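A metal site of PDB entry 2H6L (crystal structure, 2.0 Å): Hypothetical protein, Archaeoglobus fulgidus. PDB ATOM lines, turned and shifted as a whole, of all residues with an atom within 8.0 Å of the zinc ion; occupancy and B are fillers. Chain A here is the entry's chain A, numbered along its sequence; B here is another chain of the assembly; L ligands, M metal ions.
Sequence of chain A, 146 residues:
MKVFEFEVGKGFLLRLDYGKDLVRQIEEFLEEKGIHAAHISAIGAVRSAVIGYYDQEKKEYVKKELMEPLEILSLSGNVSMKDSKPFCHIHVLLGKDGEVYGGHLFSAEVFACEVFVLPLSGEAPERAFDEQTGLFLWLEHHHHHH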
ATOM      1  N   GLY A  52      -5.264 -10.349  -5.841  1.00  0.00           N
ATOM      2  CA  GLY A  52      -4.582  -9.333  -5.056  1.00  0.00           C
ATOM      3  C   GLY A  52      -4.188  -8.138  -5.872  1.00  0.00           C
ATOM      4  O   GLY A  52      -4.222  -8.163  -7.101  1.00  0.00           O
ATOM      5  N   TYR A  53      -3.827  -7.057  -5.191  1.00  0.00           N
ATOM      6  CA  TYR A  53      -3.412  -5.862  -5.889  1.00  0.00           C
ATOM      7  C   TYR A  53      -2.027  -5.490  -5.370  1.00  0.00           C
ATOM      8  O   TYR A  53      -1.665  -5.817  -4.239  1.00  0.00           O
ATOM      9  CB  TYR A  53      -4.423  -4.737  -5.694  1.00  0.00           C
ATOM     10  CG  TYR A  53      -4.589  -4.242  -4.287  1.00  0.00           C
ATOM     11  CD1 TYR A  53      -3.704  -3.301  -3.753  1.00  0.00           C
ATOM     12  CD2 TYR A  53      -5.648  -4.678  -3.492  1.00  0.00           C
ATOM     13  CE1 TYR A  53      -3.886  -2.793  -2.465  1.00  0.00           C
ATOM     14  CE2 TYR A  53      -5.837  -4.182  -2.204  1.00  0.00           C
ATOM     15  CZ  TYR A  53      -4.954  -3.233  -1.705  1.00  0.00           C
ATOM     16  OH  TYR A  53      -5.154  -2.708  -0.449  1.00  0.00           O
ATOM     17  N   TYR A  54      -1.251  -4.805  -6.200  1.00  0.00           N
ATOM     18  CA  TYR A  54       0.096  -4.426  -5.840  1.00  0.00           C
ATOM     19  C   TYR A  54       0.209  -3.006  -5.281  1.00  0.00           C
ATOM     20  O   TYR A  54      -0.125  -2.027  -5.952  1.00  0.00           O
ATOM     21  CB  TYR A  54       0.991  -4.563  -7.069  1.00  0.00           C
ATOM     22  CG  TYR A  54       2.472  -4.522  -6.775  1.00  0.00           C
ATOM     23  CD1 TYR A  54       3.085  -5.525  -6.035  1.00  0.00           C
ATOM     24  CD2 TYR A  54       3.267  -3.469  -7.253  1.00  0.00           C
ATOM     25  CE1 TYR A  54       4.457  -5.497  -5.775  1.00  0.00           C
ATOM     26  CE2 TYR A  54       4.633  -3.429  -6.999  1.00  0.00           C
ATOM     27  CZ  TYR A  54       5.231  -4.440  -6.256  1.00  0.00           C
ATOM     28  OH  TYR A  54       6.577  -4.407  -6.028  1.00  0.00           O
ATOM     29  N   TYR A  61       2.525  -7.184  -2.680  1.00  0.00           N
ATOM     30  CA  TYR A  61       1.162  -7.554  -3.024  1.00  0.00           C
ATOM     31  C   TYR A  61       0.268  -7.580  -1.789  1.00  0.00           C
ATOM     32  O   TYR A  61       0.735  -7.763  -0.660  1.00  0.00           O
ATOM     33  CB  TYR A  61       1.143  -8.910  -3.715  1.00  0.00           C
ATOM     34  CG  TYR A  61       1.504  -8.860  -5.188  1.00  0.00           C
ATOM     35  CD1 TYR A  61       0.608  -8.329  -6.116  1.00  0.00           C
ATOM     36  CD2 TYR A  61       2.718  -9.345  -5.640  1.00  0.00           C
ATOM     37  CE1 TYR A  61       0.926  -8.290  -7.476  1.00  0.00           C
ATOM     38  CE2 TYR A  61       3.045  -9.311  -7.000  1.00  0.00           C
ATOM     39  CZ  TYR A  61       2.142  -8.776  -7.913  1.00  0.00           C
ATOM     40  OH  TYR A  61       2.447  -8.746  -9.256  1.00  0.00           O
ATOM     41  N   CYS A  88       3.424 -18.193 -15.407  1.00  0.00           N
ATOM     42  CA  CYS A  88       2.203 -17.483 -15.809  1.00  0.00           C
ATOM     43  C   CYS A  88       1.965 -16.205 -15.010  1.00  0.00           C
ATOM     44  O   CYS A  88       2.107 -16.192 -13.785  1.00  0.00           O
ATOM     45  CB  CYS A  88       0.970 -18.380 -15.656  1.00  0.00           C
ATOM     46  SG  CYS A  88       0.872 -19.828 -16.734  1.00  0.00           S
ATOM     47  N   HIS A  89       1.623 -15.126 -15.717  1.00  0.00           N
ATOM     48  CA  HIS A  89       1.285 -13.855 -15.111  1.00  0.00           C
ATOM     49  C   HIS A  89      -0.122 -13.604 -15.601  1.00  0.00           C
ATOM     50  O   HIS A  89      -0.331 -13.284 -16.770  1.00  0.00           O
ATOM     51  CB  HIS A  89       2.190 -12.727 -15.609  1.00  0.00           C
ATOM     52  CG  HIS A  89       1.898 -11.408 -14.971  1.00  0.00           C
ATOM     53  ND1 HIS A  89       2.510 -10.232 -15.371  1.00  0.00           N
ATOM     54  CD2 HIS A  89       1.062 -11.076 -13.963  1.00  0.00           C
ATOM     55  CE1 HIS A  89       2.060  -9.242 -14.626  1.00  0.00           C
ATOM     56  NE2 HIS A  89       1.176  -9.718 -13.767  1.00  0.00           N
ATOM     57  N   ILE A  90      -1.094 -13.735 -14.711  1.00  0.00           N
ATOM     58  CA  ILE A  90      -2.487 -13.570 -15.108  1.00  0.00           C
ATOM     59  C   ILE A  90      -3.290 -12.596 -14.272  1.00  0.00           C
ATOM     60  O   ILE A  90      -3.180 -12.557 -13.047  1.00  0.00           O
ATOM     61  CB  ILE A  90      -3.221 -14.933 -15.043  1.00  0.00           C
ATOM     62  CG1 ILE A  90      -2.470 -15.958 -15.873  1.00  0.00           C
ATOM     63  CG2 ILE A  90      -4.666 -14.773 -15.518  1.00  0.00           C
ATOM     64  CD1 ILE A  90      -2.890 -17.393 -15.589  1.00  0.00           C
ATOM     65  N   HIS A  91      -4.120 -11.809 -14.947  1.00  0.00           N
ATOM     66  CA  HIS A  91      -4.995 -10.865 -14.273  1.00  0.00           C
ATOM     67  C   HIS A  91      -6.415 -11.308 -14.576  1.00  0.00           C
ATOM     68  O   HIS A  91      -6.700 -11.796 -15.668  1.00  0.00           O
ATOM     69  CB  HIS A  91      -4.742  -9.433 -14.754  1.00  0.00           C
ATOM     70  CG  HIS A  91      -3.574  -8.770 -14.100  1.00  0.00           C
ATOM     71  ND1 HIS A  91      -3.439  -7.403 -14.013  1.00  0.00           N
ATOM     72  CD2 HIS A  91      -2.494  -9.294 -13.464  1.00  0.00           C
ATOM     73  CE1 HIS A  91      -2.330  -7.106 -13.362  1.00  0.00           C
ATOM     74  NE2 HIS A  91      -1.746  -8.238 -13.010  1.00  0.00           N
ATOM     75  N   VAL A  92      -7.309 -11.147 -13.604  1.00  0.00           N
ATOM     76  CA  VAL A  92      -8.689 -11.568 -13.818  1.00  0.00           C
ATOM     77  C   VAL A  92      -9.730 -10.640 -13.241  1.00  0.00           C
ATOM     78  O   VAL A  92      -9.441  -9.742 -12.444  1.00  0.00           O
ATOM     79  CB  VAL A  92      -8.988 -12.945 -13.191  1.00  0.00           C
ATOM     80  CG1 VAL A  92      -8.155 -14.027 -13.851  1.00  0.00           C
ATOM     81  CG2 VAL A  92      -8.711 -12.893 -11.677  1.00  0.00           C
ATOM     82  N   GLY A 103      -8.042  -8.370 -10.169  1.00  0.00           N
ATOM     83  CA  GLY A 103      -6.662  -8.242  -9.733  1.00  0.00           C
ATOM     84  C   GLY A 103      -5.704  -9.261 -10.295  1.00  0.00           C
ATOM     85  O   GLY A 103      -5.996  -9.968 -11.253  1.00  0.00           O
ATOM     86  N   HIS A 104      -4.530  -9.310  -9.671  1.00  0.00           N
ATOM     87  CA  HIS A 104      -3.484 -10.242 -10.027  1.00  0.00           C
ATOM     88  C   HIS A 104      -4.001 -11.597  -9.508  1.00  0.00           C
ATOM     89  O   HIS A 104      -4.476 -11.693  -8.378  1.00  0.00           O
ATOM     90  CB  HIS A 104      -2.192  -9.858  -9.291  1.00  0.00           C
ATOM     91  CG  HIS A 104      -1.008 -10.720  -9.622  1.00  0.00           C
ATOM     92  ND1 HIS A 104      -0.074 -10.373 -10.567  1.00  0.00           N
ATOM     93  CD2 HIS A 104      -0.632 -11.932  -9.135  1.00  0.00           C
ATOM     94  CE1 HIS A 104       0.832 -11.329 -10.658  1.00  0.00           C
ATOM     95  NE2 HIS A 104       0.512 -12.288  -9.798  1.00  0.00           N
ATOM     96  N   LEU A 105      -3.918 -12.626 -10.341  1.00  0.00           N
ATOM     97  CA  LEU A 105      -4.412 -13.942  -9.946  1.00  0.00           C
ATOM     98  C   LEU A 105      -3.316 -14.800  -9.316  1.00  0.00           C
ATOM     99  O   LEU A 105      -2.239 -14.960  -9.880  1.00  0.00           O
ATOM    100  CB  LEU A 105      -4.979 -14.673 -11.171  1.00  0.00           C
ATOM    101  CG  LEU A 105      -5.462 -16.099 -10.941  1.00  0.00           C
ATOM    102  CD1 LEU A 105      -6.678 -16.075 -10.018  1.00  0.00           C
ATOM    103  CD2 LEU A 105      -5.820 -16.734 -12.287  1.00  0.00           C
ATOM    104  N   PHE A 106      -3.608 -15.348  -8.131  1.00  0.00           N
ATOM    105  CA  PHE A 106      -2.644 -16.194  -7.437  1.00  0.00           C
ATOM    106  C   PHE A 106      -3.076 -17.645  -7.546  1.00  0.00           C
ATOM    107  O   PHE A 106      -2.260 -18.525  -7.849  1.00  0.00           O
ATOM    108  CB  PHE A 106      -2.539 -15.794  -5.971  1.00  0.00           C
ATOM    109  CG  PHE A 106      -1.819 -14.487  -5.757  1.00  0.00           C
ATOM    110  CD1 PHE A 106      -0.439 -14.413  -5.912  1.00  0.00           C
ATOM    111  CD2 PHE A 106      -2.510 -13.342  -5.410  1.00  0.00           C
ATOM    112  CE1 PHE A 106       0.236 -13.211  -5.740  1.00  0.00           C
ATOM    113  CE2 PHE A 106      -1.839 -12.130  -5.230  1.00  0.00           C
ATOM    114  CZ  PHE A 106      -0.469 -12.067  -5.398  1.00  0.00           C
ATOM    115  N   ARG A 127      12.076 -13.148 -16.411  1.00  0.00           N
ATOM    116  CA  ARG A 127      11.726 -12.212 -15.347  1.00  0.00           C
ATOM    117  C   ARG A 127      12.861 -12.070 -14.327  1.00  0.00           C
ATOM    118  O   ARG A 127      13.324 -13.060 -13.749  1.00  0.00           O
ATOM    119  CB  ARG A 127      10.438 -12.668 -14.646  1.00  0.00           C
ATOM    120  CG  ARG A 127       9.186 -12.477 -15.501  1.00  0.00           C
ATOM    121  CD  ARG A 127       7.916 -12.926 -14.788  1.00  0.00           C
ATOM    122  NE  ARG A 127       6.751 -12.802 -15.660  1.00  0.00           N
ATOM    123  CZ  ARG A 127       6.189 -11.650 -16.014  1.00  0.00           C
ATOM    124  NH1 ARG A 127       6.688 -10.502 -15.559  1.00  0.00           N
ATOM    125  NH2 ARG A 127       5.147 -11.634 -16.831  1.00  0.00           N
ATOM    126  N   LEU A 135       9.063  -5.384  -8.668  1.00  0.00           N
ATOM    127  CA  LEU A 135       8.423  -6.494  -9.371  1.00  0.00           C
ATOM    128  C   LEU A 135       9.489  -7.281 -10.131  1.00  0.00           C
ATOM    129  O   LEU A 135      10.634  -6.860 -10.231  1.00  0.00           O
ATOM    130  CB  LEU A 135       7.416  -5.894 -10.358  1.00  0.00           C
ATOM    131  CG  LEU A 135       5.967  -6.370 -10.464  1.00  0.00           C
ATOM    132  CD1 LEU A 135       5.366  -6.604  -9.085  1.00  0.00           C
ATOM    133  CD2 LEU A 135       5.191  -5.298 -11.226  1.00  0.00           C
ATOM    134  N   ILE B  43      -1.762  -6.407 -19.484  1.00  0.00           N
ATOM    135  CA  ILE B  43      -2.040  -6.498 -18.062  1.00  0.00           C
ATOM    136  C   ILE B  43      -0.900  -5.784 -17.343  1.00  0.00           C
ATOM    137  O   ILE B  43       0.135  -5.498 -17.934  1.00  0.00           O
ATOM    138  CB  ILE B  43      -2.106  -7.963 -17.548  1.00  0.00           C
ATOM    139  CG1 ILE B  43      -0.753  -8.656 -17.738  1.00  0.00           C
ATOM    140  CG2 ILE B  43      -3.211  -8.737 -18.268  1.00  0.00           C
ATOM    141  CD1 ILE B  43      -0.703 -10.043 -17.087  1.00  0.00           C
ATOM    142  N   GLY B  44      -1.087  -5.510 -16.060  1.00  0.00           N
ATOM    143  CA  GLY B  44      -0.054  -4.824 -15.318  1.00  0.00           C
ATOM    144  C   GLY B  44      -0.684  -3.830 -14.365  1.00  0.00           C
ATOM    145  O   GLY B  44      -1.700  -4.134 -13.742  1.00  0.00           O
ATOM    146  N   ALA B  45      -0.080  -2.656 -14.241  1.00  0.00           N
ATOM    147  CA  ALA B  45      -0.596  -1.624 -13.354  1.00  0.00           C
ATOM    148  C   ALA B  45      -0.226  -0.242 -13.869  1.00  0.00           C
ATOM    149  O   ALA B  45       0.748  -0.080 -14.594  1.00  0.00           O
ATOM    150  CB  ALA B  45      -0.033  -1.834 -11.940  1.00  0.00           C
ATOM    151  N   GLU B  71      -4.640  -1.515 -10.823  1.00  0.00           N
ATOM    152  CA  GLU B  71      -4.157  -2.670 -11.568  1.00  0.00           C
ATOM    153  C   GLU B  71      -4.886  -2.614 -12.899  1.00  0.00           C
ATOM    154  O   GLU B  71      -6.024  -2.151 -12.969  1.00  0.00           O
ATOM    155  CB  GLU B  71      -4.563  -3.968 -10.878  1.00  0.00           C
ATOM    156  CG  GLU B  71      -4.015  -4.179  -9.484  1.00  0.00           C
ATOM    157  CD  GLU B  71      -2.608  -4.710  -9.509  1.00  0.00           C
ATOM    158  OE1 GLU B  71      -2.384  -5.724 -10.199  1.00  0.00           O
ATOM    159  OE2 GLU B  71      -1.732  -4.109  -8.855  1.00  0.00           O
ATOM    160  N   ILE B  72      -4.220  -3.063 -13.958  1.00  0.00           N
ATOM    161  CA  ILE B  72      -4.873  -3.130 -15.250  1.00  0.00           C
ATOM    162  C   ILE B  72      -5.536  -4.500 -15.153  1.00  0.00           C
ATOM    163  O   ILE B  72      -4.901  -5.526 -15.356  1.00  0.00           O
ATOM    164  CB  ILE B  72      -3.847  -3.144 -16.407  1.00  0.00           C
ATOM    165  CG1 ILE B  72      -2.957  -1.898 -16.345  1.00  0.00           C
ATOM    166  CG2 ILE B  72      -4.589  -3.187 -17.748  1.00  0.00           C
ATOM    167  CD1 ILE B  72      -1.824  -1.918 -17.348  1.00  0.00           C
ATOM    168  N   ALA B 112       3.913  -0.635 -14.516  1.00  0.00           N
ATOM    169  CA  ALA B 112       4.504  -1.830 -15.122  1.00  0.00           C
ATOM    170  C   ALA B 112       3.433  -2.372 -16.065  1.00  0.00           C
ATOM    171  O   ALA B 112       2.311  -2.655 -15.639  1.00  0.00           O
ATOM    172  CB  ALA B 112       4.847  -2.873 -14.077  1.00  0.00           C
ATOM    173  N   GLU B 114       2.785  -5.059 -19.544  1.00  0.00           N
ATOM    174  CA  GLU B 114       3.226  -6.076 -20.498  1.00  0.00           C
ATOM    175  C   GLU B 114       2.121  -6.178 -21.541  1.00  0.00           C
ATOM    176  O   GLU B 114       1.000  -6.581 -21.236  1.00  0.00           O
ATOM    177  CB  GLU B 114       3.440  -7.406 -19.769  1.00  0.00           C
ATOM    178  CG  GLU B 114       4.335  -7.260 -18.547  1.00  0.00           C
ATOM    179  CD  GLU B 114       4.546  -8.554 -17.759  1.00  0.00           C
ATOM    180  OE1 GLU B 114       3.621  -9.403 -17.723  1.00  0.00           O
ATOM    181  OE2 GLU B 114       5.626  -8.714 -17.170  1.00  0.00           O
HETATM  182  C1  LIG L   1       1.003  -6.316 -11.011  1.00  0.00           C
HETATM  183  O1  LIG L   1       0.127  -7.040 -10.596  1.00  0.00           O
HETATM  184  O2  LIG L   1       1.605  -5.431 -10.191  1.00  0.00           O
HETATM  185  C2  LIG L   1       1.421  -6.402 -12.449  1.00  0.00           C
HETATM  186 ZN    ZN M   1       0.142  -8.825 -12.039  1.00  0.00          ZN
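OH of Tyr 61 lies close to ND1 of His 104, 3.3 Å away.
The backbone carbonyl oxygen (O) of Gly 52 sits at hydrogen-bond distance from the backbone NH (N) of His 104 (2.8 Å).
The backbone carbonyl oxygen (O) of Ile 72 of chain B sits at hydrogen-bond distance from a ring nitrogen (ND1) of His 91, at 2.7 Å.
A ring nitrogen (ND1) of His 89 lies within hydrogen-bond range of the side-chain carboxylate of Glu 114 of chain B (2.7 Å).
The guanidinium group (NH2) of Arg 127 lies within hydrogen-bond range of a ring nitrogen (ND1) of His 89.
Merely in contact with the zinc ion: Tyr 61 (3.6 Å).
Four residues have an atom within 4 Å of the zinc ion: Tyr 61, His 89, His 91 and His 104.
Along chain A the residues within 4 Å of the zinc ion span positions 61 to 104.
The nearest printed residue that does not touch the zinc ion is Glu 71 of chain B (4.4 Å).
The zinc ion is bound by a ring nitrogen (ND1) of His 104 (2.1 Å), a ring nitrogen (NE2) of His 91 (2.2 Å), a ring nitrogen (NE2) of His 89 (2.2 Å) and an oxygen (O1) of the ligand (2.3 Å).
The zinc ion has four donor atoms within binding distance.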
